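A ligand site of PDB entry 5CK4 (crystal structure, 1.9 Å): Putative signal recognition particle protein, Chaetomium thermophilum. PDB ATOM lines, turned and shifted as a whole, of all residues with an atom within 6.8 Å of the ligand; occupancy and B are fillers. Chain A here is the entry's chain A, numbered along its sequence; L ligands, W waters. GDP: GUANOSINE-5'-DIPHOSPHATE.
The backbone NH (N) of Gly 29 is in hydrogen-bond range of an oxygen (O3B) of the ligand (2.7 Å).
N1 of the ligand sits at hydrogen-bond distance from OD1 of Asp 222, at 2.7 Å.
The backbone NH (N) of Lys 32 is in hydrogen-bond range of an oxygen (O2B) of the ligand, at 2.8 Å.
The side-chain amino group (NZ) of Lys 32 lies within salt-bridge range of an oxygen (O2B) of the ligand (2.7 Å).
The backbone NH of Val 298 lies within hydrogen-bond range of an oxygen (O6) of the ligand, at 2.7 Å.
The backbone NH of Ala 34 lies within hydrogen-bond range of an oxygen (O1A) of the ligand (2.8 Å).
N of Thr 33 lies within hydrogen-bond range of O1B of the ligand, 2.9 Å away.
O1B of the ligand is in hydrogen-bond range of OG1 of Thr 33, at 2.8 Å.
O4' of the ligand lies within hydrogen-bond range of NZ of Lys 220 (3.0 Å).
The backbone NH (N) of Gly 31 lies within hydrogen-bond range of an oxygen (O3A) of the ligand, at 3.0 Å.
An oxygen (O6) of the ligand sits close to the side-chain amide oxygen (OD1) of Asn 219, at 3.1 Å.
N of Ala 30 lies within hydrogen-bond range of O2B of the ligand, 3.2 Å away.
O6 of the ligand is in hydrogen-bond range of N of Ile 299 (3.4 Å).
NZ of Lys 32 is in hydrogen-bond range of O of Pro 27, at 3.3 Å.
The backbone carbonyl oxygen of Gly 26 sits at hydrogen-bond distance from the side-chain amino group of Lys 32, 3.3 Å away.
The backbone NH (N) of Val 298 is in hydrogen-bond range of the side-chain amide oxygen (OD1) of Asn 219, at 3.4 Å.
The backbone NH (N) of Lys 220 lies within hydrogen-bond range of the backbone carbonyl oxygen (O) of Gly 296, 3.2 Å away.
The side-chain amino group of Lys 220 lies within salt-bridge range of the side-chain carboxylate of Asp 170 (3.0 Å).
The backbone carbonyl oxygen (O) of Ala 30 lies within hydrogen-bond range of the side-chain amide nitrogen (ND2) of Asn 219.
The backbone carbonyl oxygen (O) of Ile 299 sits at hydrogen-bond distance from the side-chain amide nitrogen (ND2) of Asn 297, at 2.9 Å.
The backbone carbonyl oxygen of Gly 300 lies within hydrogen-bond range of the side-chain amide nitrogen of Asn 297.
Pro 27 touches the ligand.
Ser 28 touches the ligand (C to O3B, 3.7 Å).
Leu 223 touches the ligand.
Asn 297 touches the ligand (CA to O6, 3.5 Å).
Of the 26 residues printed, 15 come within 4 Å of the ligand.
Water W11 bridges the side-chain hydroxyl (OG1) of Thr 33 and an oxygen (O2A) of the ligand.
Water W5 lies within hydrogen-bond range of O1B of the ligand (3.0 Å) and OD1 of Asp 115 (3.2 Å).
Water W3 lies within hydrogen-bond range of the side-chain amino group of Lys 220 (2.9 Å) and a nitrogen (N3) of the ligand (3.2 Å).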
ATOM      1  N   GLY A  26      10.124  11.624 -17.515  1.00  0.00           N
ATOM      2  CA  GLY A  26      10.611  11.498 -18.876  1.00  0.00           C
ATOM      3  C   GLY A  26       9.887  12.426 -19.832  1.00  0.00           C
ATOM      4  O   GLY A  26       8.856  12.993 -19.470  1.00  0.00           O
ATOM      5  N   PRO A  27      10.422  12.578 -21.054  1.00  0.00           N
ATOM      6  CA  PRO A  27       9.765  13.477 -22.010  1.00  0.00           C
ATOM      7  C   PRO A  27       8.414  12.928 -22.435  1.00  0.00           C
ATOM      8  O   PRO A  27       8.180  11.715 -22.318  1.00  0.00           O
ATOM      9  CB  PRO A  27      10.723  13.493 -23.197  1.00  0.00           C
ATOM     10  CG  PRO A  27      11.463  12.181 -23.109  1.00  0.00           C
ATOM     11  CD  PRO A  27      11.573  11.868 -21.633  1.00  0.00           C
ATOM     12  N   SER A  28       7.535  13.796 -22.918  1.00  0.00           N
ATOM     13  CA  SER A  28       6.255  13.348 -23.433  1.00  0.00           C
ATOM     14  C   SER A  28       6.438  12.313 -24.548  1.00  0.00           C
ATOM     15  O   SER A  28       7.396  12.394 -25.305  1.00  0.00           O
ATOM     16  CB  SER A  28       5.464  14.541 -23.956  1.00  0.00           C
ATOM     17  OG  SER A  28       5.221  15.472 -22.917  1.00  0.00           O
ATOM     18  N   GLY A  29       5.512  11.366 -24.643  1.00  0.00           N
ATOM     19  CA  GLY A  29       5.577  10.321 -25.662  1.00  0.00           C
ATOM     20  C   GLY A  29       6.457   9.134 -25.285  1.00  0.00           C
ATOM     21  O   GLY A  29       6.580   8.182 -26.039  1.00  0.00           O
ATOM     22  N   ALA A  30       7.085   9.198 -24.118  1.00  0.00           N
ATOM     23  CA  ALA A  30       8.000   8.134 -23.713  1.00  0.00           C
ATOM     24  C   ALA A  30       7.229   6.850 -23.428  1.00  0.00           C
ATOM     25  O   ALA A  30       7.767   5.748 -23.601  1.00  0.00           O
ATOM     26  CB  ALA A  30       8.774   8.528 -22.493  1.00  0.00           C
ATOM     27  N   GLY A  31       5.981   6.995 -22.990  1.00  0.00           N
ATOM     28  CA  GLY A  31       5.150   5.868 -22.594  1.00  0.00           C
ATOM     29  C   GLY A  31       4.825   5.857 -21.108  1.00  0.00           C
ATOM     30  O   GLY A  31       4.508   4.809 -20.540  1.00  0.00           O
ATOM     31  N   LYS A  32       4.888   7.013 -20.451  1.00  0.00           N
ATOM     32  CA  LYS A  32       4.639   7.072 -19.015  1.00  0.00           C
ATOM     33  C   LYS A  32       3.199   6.666 -18.650  1.00  0.00           C
ATOM     34  O   LYS A  32       2.988   5.863 -17.745  1.00  0.00           O
ATOM     35  CB  LYS A  32       4.993   8.453 -18.450  1.00  0.00           C
ATOM     36  CG  LYS A  32       6.485   8.816 -18.625  1.00  0.00           C
ATOM     37  CD  LYS A  32       6.875  10.103 -17.918  1.00  0.00           C
ATOM     38  CE  LYS A  32       6.064  11.295 -18.410  1.00  0.00           C
ATOM     39  NZ  LYS A  32       6.001  11.394 -19.907  1.00  0.00           N
ATOM     40  N   THR A  33       2.221   7.206 -19.373  1.00  0.00           N
ATOM     41  CA  THR A  33       0.821   6.870 -19.121  1.00  0.00           C
ATOM     42  C   THR A  33       0.593   5.378 -19.329  1.00  0.00           C
ATOM     43  O   THR A  33      -0.035   4.705 -18.510  1.00  0.00           O
ATOM     44  CB  THR A  33      -0.150   7.671 -20.022  1.00  0.00           C
ATOM     45  OG1 THR A  33       0.073   9.079 -19.842  1.00  0.00           O
ATOM     46  CG2 THR A  33      -1.606   7.336 -19.688  1.00  0.00           C
ATOM     47  N   ALA A  34       1.140   4.868 -20.433  1.00  0.00           N
ATOM     48  CA  ALA A  34       1.016   3.446 -20.753  1.00  0.00           C
ATOM     49  C   ALA A  34       1.638   2.555 -19.675  1.00  0.00           C
ATOM     50  O   ALA A  34       1.058   1.540 -19.287  1.00  0.00           O
ATOM     51  CB  ALA A  34       1.651   3.161 -22.118  1.00  0.00           C
ATOM     52  N   LEU A  35       2.819   2.940 -19.205  1.00  0.00           N
ATOM     53  CA  LEU A  35       3.515   2.189 -18.166  1.00  0.00           C
ATOM     54  C   LEU A  35       2.725   2.162 -16.859  1.00  0.00           C
ATOM     55  O   LEU A  35       2.602   1.118 -16.237  1.00  0.00           O
ATOM     56  CB  LEU A  35       4.911   2.757 -17.923  1.00  0.00           C
ATOM     57  CG  LEU A  35       5.850   1.991 -16.990  1.00  0.00           C
ATOM     58  CD1 LEU A  35       6.073   0.560 -17.469  1.00  0.00           C
ATOM     59  CD2 LEU A  35       7.165   2.733 -16.881  1.00  0.00           C
ATOM     60  N   ASP A 115       3.411   9.132 -11.759  1.00  0.00           N
ATOM     61  CA  ASP A 115       3.531   9.737 -13.077  1.00  0.00           C
ATOM     62  C   ASP A 115       3.750  11.237 -12.913  1.00  0.00           C
ATOM     63  O   ASP A 115       3.165  11.847 -12.036  1.00  0.00           O
ATOM     64  CB  ASP A 115       2.238   9.462 -13.861  1.00  0.00           C
ATOM     65  CG  ASP A 115       2.360   9.803 -15.321  1.00  0.00           C
ATOM     66  OD1 ASP A 115       3.489   9.993 -15.806  1.00  0.00           O
ATOM     67  OD2 ASP A 115       1.314   9.861 -15.989  1.00  0.00           O
ATOM     68  N   THR A 116       4.630  11.826 -13.725  1.00  0.00           N
ATOM     69  CA  THR A 116       4.889  13.266 -13.709  1.00  0.00           C
ATOM     70  C   THR A 116       4.775  13.795 -15.133  1.00  0.00           C
ATOM     71  O   THR A 116       4.941  13.042 -16.090  1.00  0.00           O
ATOM     72  CB  THR A 116       6.290  13.612 -13.163  1.00  0.00           C
ATOM     73  OG1 THR A 116       7.291  12.982 -13.985  1.00  0.00           O
ATOM     74  CG2 THR A 116       6.434  13.124 -11.739  1.00  0.00           C
ATOM     75  N   GLY A 118       5.582  15.470 -18.716  1.00  0.00           N
ATOM     76  CA  GLY A 118       6.777  15.526 -19.536  1.00  0.00           C
ATOM     77  C   GLY A 118       7.047  16.885 -20.163  1.00  0.00           C
ATOM     78  O   GLY A 118       8.162  17.137 -20.603  1.00  0.00           O
ATOM     79  N   LEU A 168      12.042   7.339 -18.071  1.00  0.00           N
ATOM     80  CA  LEU A 168      11.595   6.612 -19.253  1.00  0.00           C
ATOM     81  C   LEU A 168      11.848   7.428 -20.514  1.00  0.00           C
ATOM     82  O   LEU A 168      11.593   8.626 -20.541  1.00  0.00           O
ATOM     83  CB  LEU A 168      10.100   6.323 -19.151  1.00  0.00           C
ATOM     84  CG  LEU A 168       9.421   5.272 -20.045  1.00  0.00           C
ATOM     85  CD1 LEU A 168       9.859   3.852 -19.660  1.00  0.00           C
ATOM     86  CD2 LEU A 168       7.919   5.391 -19.916  1.00  0.00           C
ATOM     87  N   ASP A 170      11.861   7.037 -25.137  1.00  0.00           N
ATOM     88  CA  ASP A 170      11.494   6.290 -26.344  1.00  0.00           C
ATOM     89  C   ASP A 170      12.779   5.867 -27.065  1.00  0.00           C
ATOM     90  O   ASP A 170      13.443   6.688 -27.677  1.00  0.00           O
ATOM     91  CB  ASP A 170      10.625   7.197 -27.233  1.00  0.00           C
ATOM     92  CG  ASP A 170      10.115   6.503 -28.477  1.00  0.00           C
ATOM     93  OD1 ASP A 170      10.670   5.460 -28.865  1.00  0.00           O
ATOM     94  OD2 ASP A 170       9.150   7.014 -29.076  1.00  0.00           O
ATOM     95  N   ASN A 219      12.458   2.347 -23.307  1.00  0.00           N
ATOM     96  CA  ASN A 219      11.165   1.787 -23.697  1.00  0.00           C
ATOM     97  C   ASN A 219      11.012   1.573 -25.209  1.00  0.00           C
ATOM     98  O   ASN A 219      11.801   2.096 -26.003  1.00  0.00           O
ATOM     99  CB  ASN A 219      10.036   2.703 -23.208  1.00  0.00           C
ATOM    100  CG  ASN A 219       8.671   2.038 -23.236  1.00  0.00           C
ATOM    101  OD1 ASN A 219       8.567   0.814 -23.113  1.00  0.00           O
ATOM    102  ND2 ASN A 219       7.609   2.830 -23.387  1.00  0.00           N
ATOM    103  N   LYS A 220       9.962   0.832 -25.584  1.00  0.00           N
ATOM    104  CA  LYS A 220       9.584   0.557 -26.978  1.00  0.00           C
ATOM    105  C   LYS A 220      10.561  -0.379 -27.693  1.00  0.00           C
ATOM    106  O   LYS A 220      10.765  -0.258 -28.901  1.00  0.00           O
ATOM    107  CB  LYS A 220       9.323   1.856 -27.805  1.00  0.00           C
ATOM    108  CG  LYS A 220       8.481   2.919 -27.042  1.00  0.00           C
ATOM    109  CD  LYS A 220       7.831   3.944 -27.951  1.00  0.00           C
ATOM    110  CE  LYS A 220       7.129   5.041 -27.134  1.00  0.00           C
ATOM    111  NZ  LYS A 220       6.477   6.093 -27.999  1.00  0.00           N
ATOM    112  N   GLN A 221      11.167  -1.311 -26.956  1.00  0.00           N
ATOM    113  CA  GLN A 221      12.066  -2.289 -27.576  1.00  0.00           C
ATOM    114  C   GLN A 221      11.357  -3.288 -28.507  1.00  0.00           C
ATOM    115  O   GLN A 221      12.004  -4.077 -29.185  1.00  0.00           O
ATOM    116  CB  GLN A 221      12.892  -3.048 -26.522  1.00  0.00           C
ATOM    117  CG  GLN A 221      13.876  -2.174 -25.760  1.00  0.00           C
ATOM    118  CD  GLN A 221      15.026  -1.697 -26.618  1.00  0.00           C
ATOM    119  OE1 GLN A 221      15.480  -2.403 -27.511  1.00  0.00           O
ATOM    120  NE2 GLN A 221      15.526  -0.494 -26.323  1.00  0.00           N
ATOM    121  N   ASP A 222      10.031  -3.227 -28.555  1.00  0.00           N
ATOM    122  CA  ASP A 222       9.262  -4.024 -29.503  1.00  0.00           C
ATOM    123  C   ASP A 222       9.476  -3.499 -30.932  1.00  0.00           C
ATOM    124  O   ASP A 222       9.356  -4.246 -31.894  1.00  0.00           O
ATOM    125  CB  ASP A 222       7.775  -3.987 -29.152  1.00  0.00           C
ATOM    126  CG  ASP A 222       7.225  -2.566 -29.050  1.00  0.00           C
ATOM    127  OD1 ASP A 222       7.779  -1.780 -28.248  1.00  0.00           O
ATOM    128  OD2 ASP A 222       6.246  -2.245 -29.762  1.00  0.00           O
ATOM    129  N   LEU A 223       9.801  -2.217 -31.057  1.00  0.00           N
ATOM    130  CA  LEU A 223       9.962  -1.591 -32.369  1.00  0.00           C
ATOM    131  C   LEU A 223      11.281  -1.989 -32.994  1.00  0.00           C
ATOM    132  O   LEU A 223      12.315  -2.011 -32.326  1.00  0.00           O
ATOM    133  CB  LEU A 223       9.863  -0.073 -32.257  1.00  0.00           C
ATOM    134  CG  LEU A 223       8.502   0.469 -31.810  1.00  0.00           C
ATOM    135  CD1 LEU A 223       8.539   1.994 -31.656  1.00  0.00           C
ATOM    136  CD2 LEU A 223       7.433   0.075 -32.796  1.00  0.00           C
ATOM    137  N   GLY A 296      13.266  -2.339 -22.328  1.00  0.00           N
ATOM    138  CA  GLY A 296      11.981  -2.986 -22.099  1.00  0.00           C
ATOM    139  C   GLY A 296      10.921  -2.448 -23.021  1.00  0.00           C
ATOM    140  O   GLY A 296      11.216  -1.629 -23.908  1.00  0.00           O
ATOM    141  N   ASN A 297       9.690  -2.901 -22.836  1.00  0.00           N
ATOM    142  CA  ASN A 297       8.562  -2.429 -23.625  1.00  0.00           C
ATOM    143  C   ASN A 297       7.248  -2.630 -22.869  1.00  0.00           C
ATOM    144  O   ASN A 297       7.103  -3.592 -22.105  1.00  0.00           O
ATOM    145  CB  ASN A 297       8.532  -3.100 -25.004  1.00  0.00           C
ATOM    146  CG  ASN A 297       8.370  -4.613 -24.903  1.00  0.00           C
ATOM    147  OD1 ASN A 297       9.285  -5.323 -24.507  1.00  0.00           O
ATOM    148  ND2 ASN A 297       7.184  -5.108 -25.268  1.00  0.00           N
ATOM    149  N   VAL A 298       6.299  -1.724 -23.083  1.00  0.00           N
ATOM    150  CA  VAL A 298       5.007  -1.769 -22.414  1.00  0.00           C
ATOM    151  C   VAL A 298       3.977  -2.513 -23.267  1.00  0.00           C
ATOM    152  O   VAL A 298       3.086  -3.184 -22.733  1.00  0.00           O
ATOM    153  CB  VAL A 298       4.495  -0.336 -22.106  1.00  0.00           C
ATOM    154  CG1 VAL A 298       3.122  -0.368 -21.483  1.00  0.00           C
ATOM    155  CG2 VAL A 298       5.474   0.377 -21.183  1.00  0.00           C
ATOM    156  N   ILE A 299       4.102  -2.412 -24.584  1.00  0.00           N
ATOM    157  CA  ILE A 299       3.208  -3.111 -25.500  1.00  0.00           C
ATOM    158  C   ILE A 299       4.027  -3.806 -26.567  1.00  0.00           C
ATOM    159  O   ILE A 299       5.226  -3.546 -26.686  1.00  0.00           O
ATOM    160  CB  ILE A 299       2.187  -2.150 -26.157  1.00  0.00           C
ATOM    161  CG1 ILE A 299       2.874  -1.230 -27.151  1.00  0.00           C
ATOM    162  CG2 ILE A 299       1.451  -1.333 -25.114  1.00  0.00           C
ATOM    163  CD1 ILE A 299       1.925  -0.293 -27.873  1.00  0.00           C
ATOM    164  N   GLY A 300       3.403  -4.710 -27.336  1.00  0.00           N
ATOM    165  CA  GLY A 300       4.124  -5.414 -28.392  1.00  0.00           C
ATOM    166  C   GLY A 300       4.960  -6.573 -27.899  1.00  0.00           C
ATOM    167  O   GLY A 300       5.045  -6.839 -26.707  1.00  0.00           O
ATOM    168  N   TRP A 308      12.242  -4.305 -15.283  1.00  0.00           N
ATOM    169  CA  TRP A 308      12.205  -2.976 -14.677  1.00  0.00           C
ATOM    170  C   TRP A 308      11.631  -3.067 -13.255  1.00  0.00           C
ATOM    171  O   TRP A 308      12.201  -2.509 -12.325  1.00  0.00           O
ATOM    172  CB  TRP A 308      11.337  -2.010 -15.490  1.00  0.00           C
ATOM    173  CG  TRP A 308      11.869  -1.570 -16.816  1.00  0.00           C
ATOM    174  CD1 TRP A 308      13.174  -1.526 -17.214  1.00  0.00           C
ATOM    175  CD2 TRP A 308      11.096  -1.077 -17.917  1.00  0.00           C
ATOM    176  NE1 TRP A 308      13.268  -1.048 -18.496  1.00  0.00           N
ATOM    177  CE2 TRP A 308      11.999  -0.764 -18.951  1.00  0.00           C
ATOM    178  CE3 TRP A 308       9.730  -0.900 -18.136  1.00  0.00           C
ATOM    179  CZ2 TRP A 308      11.585  -0.256 -20.187  1.00  0.00           C
ATOM    180  CZ3 TRP A 308       9.310  -0.397 -19.359  1.00  0.00           C
ATOM    181  CH2 TRP A 308      10.234  -0.080 -20.363  1.00  0.00           C
HETATM  182  PB  GDP L   1       3.550   9.688 -22.170  1.00  0.00           P
HETATM  183  O1B GDP L   1       2.604   9.575 -21.018  1.00  0.00           O
HETATM  184  O2B GDP L   1       4.979   9.563 -21.675  1.00  0.00           O
HETATM  185  O3B GDP L   1       3.440  10.994 -22.913  1.00  0.00           O
HETATM  186  O3A GDP L   1       3.348   8.493 -23.234  1.00  0.00           O
HETATM  187  PA  GDP L   1       1.991   7.656 -23.524  1.00  0.00           P
HETATM  188  O1A GDP L   1       1.702   6.712 -22.403  1.00  0.00           O
HETATM  189  O2A GDP L   1       0.829   8.541 -23.870  1.00  0.00           O
HETATM  190  O5' GDP L   1       2.569   6.866 -24.786  1.00  0.00           O
HETATM  191  C5' GDP L   1       2.909   7.567 -25.971  1.00  0.00           C
HETATM  192  C4' GDP L   1       2.657   6.645 -27.146  1.00  0.00           C
HETATM  193  O4' GDP L   1       3.640   5.600 -27.141  1.00  0.00           O
HETATM  194  C3' GDP L   1       1.295   5.967 -27.065  1.00  0.00           C
HETATM  195  O3' GDP L   1       0.815   5.830 -28.397  1.00  0.00           O
HETATM  196  C2' GDP L   1       1.610   4.583 -26.526  1.00  0.00           C
HETATM  197  O2' GDP L   1       0.691   3.587 -26.971  1.00  0.00           O
HETATM  198  C1' GDP L   1       2.969   4.330 -27.129  1.00  0.00           C
HETATM  199  N9  GDP L   1       3.766   3.358 -26.358  1.00  0.00           N
HETATM  200  C8  GDP L   1       3.967   3.327 -25.023  1.00  0.00           C
HETATM  201  N7  GDP L   1       4.792   2.290 -24.691  1.00  0.00           N
HETATM  202  C5  GDP L   1       5.124   1.668 -25.828  1.00  0.00           C
HETATM  203  C6  GDP L   1       5.943   0.508 -26.199  1.00  0.00           C
HETATM  204  O6  GDP L   1       6.552  -0.134 -25.307  1.00  0.00           O
HETATM  205  N1  GDP L   1       6.040   0.201 -27.504  1.00  0.00           N
HETATM  206  C2  GDP L   1       5.389   0.883 -28.471  1.00  0.00           C
HETATM  207  N2  GDP L   1       5.523   0.510 -29.766  1.00  0.00           N
HETATM  208  N3  GDP L   1       4.613   1.967 -28.202  1.00  0.00           N
HETATM  209  C4  GDP L   1       4.451   2.385 -26.920  1.00  0.00           C
HETATM  210  O   HOH W   1      -1.778   5.678 -28.591  1.00  0.00           O
HETATM  211  O   HOH W   2       3.845   1.283 -31.982  1.00  0.00           O
HETATM  212  O   HOH W   3       5.087   4.609 -30.018  1.00  0.00           O
HETATM  213  O   HOH W   4       1.973  11.403 -25.354  1.00  0.00           O
HETATM  214  O   HOH W   5       2.650  11.334 -18.558  1.00  0.00           O
HETATM  215  O   HOH W   6      -0.276   2.553 -29.311  1.00  0.00           O
HETATM  216  O   HOH W   7      -0.940   5.856 -23.290  1.00  0.00           O
HETATM  217  O   HOH W   8      -1.380   3.660 -24.912  1.00  0.00           O
HETATM  218  O   HOH W   9      -0.891   8.717 -26.133  1.00  0.00           O
HETATM  219  O   HOH W  10       3.124  10.052 -28.163  1.00  0.00           O
HETATM  220  O   HOH W  11      -0.437  10.645 -22.196  1.00  0.00           O
